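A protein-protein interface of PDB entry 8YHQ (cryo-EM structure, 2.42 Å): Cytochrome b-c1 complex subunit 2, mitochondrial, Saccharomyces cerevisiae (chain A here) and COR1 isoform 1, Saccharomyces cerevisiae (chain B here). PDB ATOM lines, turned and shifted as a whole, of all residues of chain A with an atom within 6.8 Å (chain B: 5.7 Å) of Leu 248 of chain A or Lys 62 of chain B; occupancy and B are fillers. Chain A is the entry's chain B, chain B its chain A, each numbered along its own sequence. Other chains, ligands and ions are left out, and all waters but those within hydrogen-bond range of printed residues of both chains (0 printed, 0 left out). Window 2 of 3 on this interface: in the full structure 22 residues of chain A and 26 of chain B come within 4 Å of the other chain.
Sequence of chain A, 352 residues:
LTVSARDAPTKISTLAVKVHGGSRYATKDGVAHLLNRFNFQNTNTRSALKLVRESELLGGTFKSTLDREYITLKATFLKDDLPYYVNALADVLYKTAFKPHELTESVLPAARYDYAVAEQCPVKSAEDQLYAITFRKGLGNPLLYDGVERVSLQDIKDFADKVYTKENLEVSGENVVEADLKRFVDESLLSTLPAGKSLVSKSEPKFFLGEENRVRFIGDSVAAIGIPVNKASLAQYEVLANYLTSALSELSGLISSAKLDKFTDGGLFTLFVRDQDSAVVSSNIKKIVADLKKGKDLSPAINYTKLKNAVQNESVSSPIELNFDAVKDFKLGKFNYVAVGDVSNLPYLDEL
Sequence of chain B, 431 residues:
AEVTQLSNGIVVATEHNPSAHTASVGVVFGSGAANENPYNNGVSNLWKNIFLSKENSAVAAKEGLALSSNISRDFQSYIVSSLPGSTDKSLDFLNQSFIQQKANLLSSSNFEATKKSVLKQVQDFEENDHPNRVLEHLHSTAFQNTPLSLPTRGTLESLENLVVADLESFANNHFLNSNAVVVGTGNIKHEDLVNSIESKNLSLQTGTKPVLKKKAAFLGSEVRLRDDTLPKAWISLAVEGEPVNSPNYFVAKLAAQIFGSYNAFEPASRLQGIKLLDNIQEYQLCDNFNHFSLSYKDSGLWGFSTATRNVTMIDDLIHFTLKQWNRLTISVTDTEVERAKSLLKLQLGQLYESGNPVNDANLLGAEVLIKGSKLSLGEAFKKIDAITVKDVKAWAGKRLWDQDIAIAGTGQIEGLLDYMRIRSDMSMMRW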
ATOM      1  N   ASN A 242      28.702  19.349  -2.577  1.00  0.00           N
ATOM      2  CA  ASN A 242      29.630  18.760  -3.531  1.00  0.00           C
ATOM      3  C   ASN A 242      29.232  19.036  -4.974  1.00  0.00           C
ATOM      4  O   ASN A 242      30.108  19.109  -5.838  1.00  0.00           O
ATOM      5  CB  ASN A 242      29.737  17.257  -3.287  1.00  0.00           C
ATOM      6  CG  ASN A 242      30.677  16.920  -2.151  1.00  0.00           C
ATOM      7  OD1 ASN A 242      31.875  17.182  -2.221  1.00  0.00           O
ATOM      8  ND2 ASN A 242      30.135  16.341  -1.092  1.00  0.00           N
ATOM      9  N   TYR A 243      27.938  19.198  -5.251  1.00  0.00           N
ATOM     10  CA  TYR A 243      27.502  19.583  -6.588  1.00  0.00           C
ATOM     11  C   TYR A 243      28.006  20.970  -6.969  1.00  0.00           C
ATOM     12  O   TYR A 243      28.466  21.179  -8.095  1.00  0.00           O
ATOM     13  CB  TYR A 243      25.978  19.530  -6.667  1.00  0.00           C
ATOM     14  CG  TYR A 243      25.395  20.074  -7.948  1.00  0.00           C
ATOM     15  CD1 TYR A 243      25.390  19.315  -9.102  1.00  0.00           C
ATOM     16  CD2 TYR A 243      24.838  21.340  -8.000  1.00  0.00           C
ATOM     17  CE1 TYR A 243      24.857  19.801 -10.270  1.00  0.00           C
ATOM     18  CE2 TYR A 243      24.306  21.834  -9.165  1.00  0.00           C
ATOM     19  CZ  TYR A 243      24.317  21.058 -10.299  1.00  0.00           C
ATOM     20  OH  TYR A 243      23.786  21.538 -11.472  1.00  0.00           O
ATOM     21  N   THR A 245      30.581  22.726  -6.071  1.00  0.00           N
ATOM     22  CA  THR A 245      32.017  22.860  -6.274  1.00  0.00           C
ATOM     23  C   THR A 245      32.553  21.980  -7.394  1.00  0.00           C
ATOM     24  O   THR A 245      33.623  22.277  -7.935  1.00  0.00           O
ATOM     25  CB  THR A 245      32.763  22.532  -4.981  1.00  0.00           C
ATOM     26  OG1 THR A 245      32.262  21.311  -4.430  1.00  0.00           O
ATOM     27  CG2 THR A 245      32.579  23.639  -3.979  1.00  0.00           C
ATOM     28  N   SER A 246      31.848  20.915  -7.751  1.00  0.00           N
ATOM     29  CA  SER A 246      32.257  20.047  -8.838  1.00  0.00           C
ATOM     30  C   SER A 246      32.153  20.760 -10.180  1.00  0.00           C
ATOM     31  O   SER A 246      31.641  21.874 -10.296  1.00  0.00           O
ATOM     32  CB  SER A 246      31.397  18.789  -8.863  1.00  0.00           C
ATOM     33  OG  SER A 246      30.148  19.052  -9.469  1.00  0.00           O
ATOM     34  N   ALA A 247      32.649  20.082 -11.211  1.00  0.00           N
ATOM     35  CA  ALA A 247      32.535  20.543 -12.586  1.00  0.00           C
ATOM     36  C   ALA A 247      31.178  20.246 -13.211  1.00  0.00           C
ATOM     37  O   ALA A 247      30.988  20.526 -14.397  1.00  0.00           O
ATOM     38  CB  ALA A 247      33.636  19.910 -13.433  1.00  0.00           C
ATOM     39  N   LEU A 248      30.239  19.680 -12.456  1.00  0.00           N
ATOM     40  CA  LEU A 248      28.888  19.493 -12.962  1.00  0.00           C
ATOM     41  C   LEU A 248      28.093  20.793 -12.996  1.00  0.00           C
ATOM     42  O   LEU A 248      27.032  20.837 -13.627  1.00  0.00           O
ATOM     43  CB  LEU A 248      28.152  18.469 -12.103  1.00  0.00           C
ATOM     44  CG  LEU A 248      28.708  17.048 -12.078  1.00  0.00           C
ATOM     45  CD1 LEU A 248      28.149  16.273 -10.902  1.00  0.00           C
ATOM     46  CD2 LEU A 248      28.405  16.333 -13.364  1.00  0.00           C
ATOM     47  N   SER A 249      28.587  21.848 -12.352  1.00  0.00           N
ATOM     48  CA  SER A 249      27.845  23.083 -12.152  1.00  0.00           C
ATOM     49  C   SER A 249      28.378  24.188 -13.053  1.00  0.00           C
ATOM     50  O   SER A 249      29.573  24.246 -13.350  1.00  0.00           O
ATOM     51  CB  SER A 249      27.932  23.532 -10.694  1.00  0.00           C
ATOM     52  OG  SER A 249      26.656  23.677 -10.115  1.00  0.00           O
ATOM     53  N   GLU A 250      27.482  25.078 -13.470  1.00  0.00           N
ATOM     54  CA  GLU A 250      27.860  26.219 -14.294  1.00  0.00           C
ATOM     55  C   GLU A 250      28.465  27.351 -13.481  1.00  0.00           C
ATOM     56  O   GLU A 250      29.233  28.149 -14.029  1.00  0.00           O
ATOM     57  CB  GLU A 250      26.654  26.777 -15.055  1.00  0.00           C
ATOM     58  CG  GLU A 250      25.940  25.807 -15.986  1.00  0.00           C
ATOM     59  CD  GLU A 250      24.999  24.845 -15.272  1.00  0.00           C
ATOM     60  OE1 GLU A 250      24.718  25.055 -14.076  1.00  0.00           O
ATOM     61  OE2 GLU A 250      24.538  23.878 -15.915  1.00  0.00           O
ATOM     62  N   LEU A 251      28.126  27.443 -12.197  1.00  0.00           N
ATOM     63  CA  LEU A 251      28.527  28.549 -11.337  1.00  0.00           C
ATOM     64  C   LEU A 251      29.560  28.113 -10.303  1.00  0.00           C
ATOM     65  O   LEU A 251      29.706  28.753  -9.259  1.00  0.00           O
ATOM     66  CB  LEU A 251      27.302  29.160 -10.652  1.00  0.00           C
ATOM     67  CG  LEU A 251      26.367  28.248  -9.857  1.00  0.00           C
ATOM     68  CD1 LEU A 251      26.837  28.042  -8.436  1.00  0.00           C
ATOM     69  CD2 LEU A 251      24.978  28.835  -9.877  1.00  0.00           C
ATOM     70  N   SER A 252      30.287  27.032 -10.583  1.00  0.00           N
ATOM     71  CA  SER A 252      31.323  26.576  -9.669  1.00  0.00           C
ATOM     72  C   SER A 252      32.573  27.437  -9.750  1.00  0.00           C
ATOM     73  O   SER A 252      33.406  27.384  -8.841  1.00  0.00           O
ATOM     74  CB  SER A 252      31.673  25.116  -9.950  1.00  0.00           C
ATOM     75  OG  SER A 252      33.045  24.960 -10.238  1.00  0.00           O
ATOM     76  N   PRO A 300      22.352  13.865 -10.769  1.00  0.00           N
ATOM     77  CA  PRO A 300      23.651  13.563 -11.391  1.00  0.00           C
ATOM     78  C   PRO A 300      24.836  13.517 -10.432  1.00  0.00           C
ATOM     79  O   PRO A 300      25.895  13.023 -10.838  1.00  0.00           O
ATOM     80  CB  PRO A 300      23.814  14.693 -12.409  1.00  0.00           C
ATOM     81  CG  PRO A 300      22.459  15.023 -12.790  1.00  0.00           C
ATOM     82  CD  PRO A 300      21.631  14.881 -11.555  1.00  0.00           C
ATOM     83  N   ALA A 301      24.702  14.000  -9.193  1.00  0.00           N
ATOM     84  CA  ALA A 301      25.817  14.108  -8.260  1.00  0.00           C
ATOM     85  C   ALA A 301      25.712  13.135  -7.089  1.00  0.00           C
ATOM     86  O   ALA A 301      26.344  13.354  -6.052  1.00  0.00           O
ATOM     87  CB  ALA A 301      25.923  15.542  -7.744  1.00  0.00           C
ATOM     88  N   ILE A 302      24.942  12.058  -7.232  1.00  0.00           N
ATOM     89  CA  ILE A 302      24.792  11.098  -6.143  1.00  0.00           C
ATOM     90  C   ILE A 302      26.042  10.239  -6.003  1.00  0.00           C
ATOM     91  O   ILE A 302      26.539  10.018  -4.894  1.00  0.00           O
ATOM     92  CB  ILE A 302      23.540  10.224  -6.362  1.00  0.00           C
ATOM     93  CG1 ILE A 302      22.267  11.076  -6.472  1.00  0.00           C
ATOM     94  CG2 ILE A 302      23.413   9.197  -5.255  1.00  0.00           C
ATOM     95  CD1 ILE A 302      21.986  11.979  -5.314  1.00  0.00           C
ATOM     96  N   ASN A 303      26.563   9.731  -7.121  1.00  0.00           N
ATOM     97  CA  ASN A 303      27.709   8.831  -7.062  1.00  0.00           C
ATOM     98  C   ASN A 303      29.009   9.586  -6.815  1.00  0.00           C
ATOM     99  O   ASN A 303      29.936   9.035  -6.214  1.00  0.00           O
ATOM    100  CB  ASN A 303      27.799   8.020  -8.352  1.00  0.00           C
ATOM    101  CG  ASN A 303      26.657   7.039  -8.502  1.00  0.00           C
ATOM    102  OD1 ASN A 303      26.224   6.415  -7.536  1.00  0.00           O
ATOM    103  ND2 ASN A 303      26.163   6.897  -9.721  1.00  0.00           N
ATOM    104  N   TYR A 304      29.096  10.835  -7.272  1.00  0.00           N
ATOM    105  CA  TYR A 304      30.263  11.660  -6.977  1.00  0.00           C
ATOM    106  C   TYR A 304      30.317  12.034  -5.500  1.00  0.00           C
ATOM    107  O   TYR A 304      31.402  12.211  -4.937  1.00  0.00           O
ATOM    108  CB  TYR A 304      30.237  12.907  -7.854  1.00  0.00           C
ATOM    109  CG  TYR A 304      31.420  13.827  -7.699  1.00  0.00           C
ATOM    110  CD1 TYR A 304      32.630  13.545  -8.306  1.00  0.00           C
ATOM    111  CD2 TYR A 304      31.318  14.991  -6.960  1.00  0.00           C
ATOM    112  CE1 TYR A 304      33.705  14.390  -8.169  1.00  0.00           C
ATOM    113  CE2 TYR A 304      32.388  15.840  -6.820  1.00  0.00           C
ATOM    114  CZ  TYR A 304      33.579  15.535  -7.430  1.00  0.00           C
ATOM    115  OH  TYR A 304      34.654  16.375  -7.297  1.00  0.00           O
ATOM    116  N   LYS B  54      37.662  21.311 -16.931  1.00  0.00           N
ATOM    117  CA  LYS B  54      36.259  21.109 -16.581  1.00  0.00           C
ATOM    118  C   LYS B  54      35.633  19.938 -17.325  1.00  0.00           C
ATOM    119  O   LYS B  54      35.087  19.028 -16.695  1.00  0.00           O
ATOM    120  CB  LYS B  54      35.468  22.387 -16.857  1.00  0.00           C
ATOM    121  CG  LYS B  54      33.980  22.320 -16.539  1.00  0.00           C
ATOM    122  CD  LYS B  54      33.560  23.344 -15.535  1.00  0.00           C
ATOM    123  CE  LYS B  54      32.088  23.184 -15.229  1.00  0.00           C
ATOM    124  NZ  LYS B  54      31.288  24.368 -15.585  1.00  0.00           N
ATOM    125  N   SER B  57      36.760  16.670 -16.082  1.00  0.00           N
ATOM    126  CA  SER B  57      36.330  16.392 -14.717  1.00  0.00           C
ATOM    127  C   SER B  57      34.820  16.244 -14.622  1.00  0.00           C
ATOM    128  O   SER B  57      34.321  15.535 -13.740  1.00  0.00           O
ATOM    129  CB  SER B  57      36.810  17.497 -13.777  1.00  0.00           C
ATOM    130  OG  SER B  57      38.216  17.577 -13.754  1.00  0.00           O
ATOM    131  N   ALA B  58      34.077  16.909 -15.506  1.00  0.00           N
ATOM    132  CA  ALA B  58      32.636  16.707 -15.574  1.00  0.00           C
ATOM    133  C   ALA B  58      32.304  15.287 -16.013  1.00  0.00           C
ATOM    134  O   ALA B  58      31.444  14.626 -15.420  1.00  0.00           O
ATOM    135  CB  ALA B  58      32.015  17.722 -16.528  1.00  0.00           C
ATOM    136  N   VAL B  59      32.978  14.805 -17.059  1.00  0.00           N
ATOM    137  CA  VAL B  59      32.731  13.462 -17.573  1.00  0.00           C
ATOM    138  C   VAL B  59      33.071  12.410 -16.529  1.00  0.00           C
ATOM    139  O   VAL B  59      32.443  11.345 -16.483  1.00  0.00           O
ATOM    140  CB  VAL B  59      33.522  13.253 -18.880  1.00  0.00           C
ATOM    141  CG1 VAL B  59      33.511  11.794 -19.300  1.00  0.00           C
ATOM    142  CG2 VAL B  59      32.950  14.111 -19.993  1.00  0.00           C
ATOM    143  N   ALA B  60      34.057  12.682 -15.675  1.00  0.00           N
ATOM    144  CA  ALA B  60      34.397  11.758 -14.600  1.00  0.00           C
ATOM    145  C   ALA B  60      33.416  11.856 -13.437  1.00  0.00           C
ATOM    146  O   ALA B  60      33.112  10.846 -12.793  1.00  0.00           O
ATOM    147  CB  ALA B  60      35.819  12.023 -14.121  1.00  0.00           C
ATOM    148  N   ALA B  61      32.912  13.057 -13.151  1.00  0.00           N
ATOM    149  CA  ALA B  61      32.001  13.235 -12.027  1.00  0.00           C
ATOM    150  C   ALA B  61      30.654  12.568 -12.272  1.00  0.00           C
ATOM    151  O   ALA B  61      30.033  12.071 -11.328  1.00  0.00           O
ATOM    152  CB  ALA B  61      31.817  14.723 -11.742  1.00  0.00           C
ATOM    153  N   LYS B  62      30.182  12.551 -13.520  1.00  0.00           N
ATOM    154  CA  LYS B  62      28.947  11.848 -13.842  1.00  0.00           C
ATOM    155  C   LYS B  62      29.047  10.352 -13.579  1.00  0.00           C
ATOM    156  O   LYS B  62      28.020   9.712 -13.332  1.00  0.00           O
ATOM    157  CB  LYS B  62      28.565  12.095 -15.300  1.00  0.00           C
ATOM    158  CG  LYS B  62      28.021  13.479 -15.560  1.00  0.00           C
ATOM    159  CD  LYS B  62      27.532  13.657 -16.987  1.00  0.00           C
ATOM    160  CE  LYS B  62      28.670  14.001 -17.938  1.00  0.00           C
ATOM    161  NZ  LYS B  62      29.169  15.388 -17.752  1.00  0.00           N
ATOM    162  N   GLU B  63      30.253   9.785 -13.623  1.00  0.00           N
ATOM    163  CA  GLU B  63      30.483   8.380 -13.324  1.00  0.00           C
ATOM    164  C   GLU B  63      30.918   8.113 -11.889  1.00  0.00           C
ATOM    165  O   GLU B  63      30.995   6.945 -11.498  1.00  0.00           O
ATOM    166  CB  GLU B  63      31.547   7.809 -14.270  1.00  0.00           C
ATOM    167  CG  GLU B  63      31.140   7.767 -15.728  1.00  0.00           C
ATOM    168  CD  GLU B  63      29.998   6.809 -15.999  1.00  0.00           C
ATOM    169  OE1 GLU B  63      29.905   5.776 -15.304  1.00  0.00           O
ATOM    170  OE2 GLU B  63      29.187   7.095 -16.902  1.00  0.00           O
ATOM    171  N   GLY B  64      31.213   9.146 -11.104  1.00  0.00           N
ATOM    172  CA  GLY B  64      31.641   8.962  -9.732  1.00  0.00           C
ATOM    173  C   GLY B  64      33.138   8.802  -9.584  1.00  0.00           C
ATOM    174  O   GLY B  64      33.603   7.958  -8.813  1.00  0.00           O
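Of chain B, only Ala 61 and Lys 62 come within 4 Å of Leu 248 of chain A.
Of the printed residues of chain A, Gly 64 of chain B touches Asn 303 (3.9 Å).
Printed residues of chain A within 4 Å of Ala 61 of chain B: Leu 248 (3.9 Å) and Tyr 304 (3.6 Å).
Of the printed residues of chain A, Lys 54 of chain B touches Ala 247 (3.0 Å) and Ser 249 (2.8 Å).
Printed residues of chain B within 4 Å of Tyr 304 of chain A: Ala 61 (3.6 Å).
Printed residues of chain A within 4 Å of Ala 58 of chain B: Ala 247 (3.7 Å).
The nearest residue of chain A that does not touch Lys 62 of chain B is Pro 300 of chain A (4.4 Å).
The backbone carbonyl oxygen (O) of Ser 249 of chain A sits at hydrogen-bond distance from the side-chain amino group (NZ) of Lys 54 of chain B (2.8 Å).
Ala 247 of chain A touches Lys 54 of chain B.
O of Ala 247 of chain A touches CB of Ala 58 of chain B (3.7 Å).
Leu 248 of chain A touches Ala 61 of chain B.
Lys 62 of chain B touches Leu 248 of chain A (CG to CD2, 3.6 Å).
O of Asn 303 of chain A touches CA of Gly 64 of chain B, 3.9 Å away.
O of Ala 61 of chain B touches CB of Tyr 304 of chain A (3.6 Å).
Printed residues of chain A that touch a printed residue of chain B: Ala 247, Leu 248, Ser 249, Asn 303 and Tyr 304.
Hydrophobic or aromatic side chains of chain A that line the printed part of chain B: Ala 247, Leu 248 and Tyr 304.
Printed residues of chain B that touch a printed residue of chain A: Lys 54, Ala 58, Ala 61, Lys 62 and Gly 64.
Hydrophobic or aromatic side chains of chain B that line the printed part of chain A: Ala 58 and Ala 61.
Among the printed residues, no Asp or Glu carboxylate lies within 4 Å of a Lys or Arg side-chain nitrogen of the other chain.
The backbone carbonyl oxygen of Ala 58 of chain B is in hydrogen-bond range of the side-chain amino group of Lys 62 of chain B.
The side-chain hydroxyl (OG) of Ser 246 of chain A is in hydrogen-bond range of the backbone NH (N) of Leu 248 of chain A.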
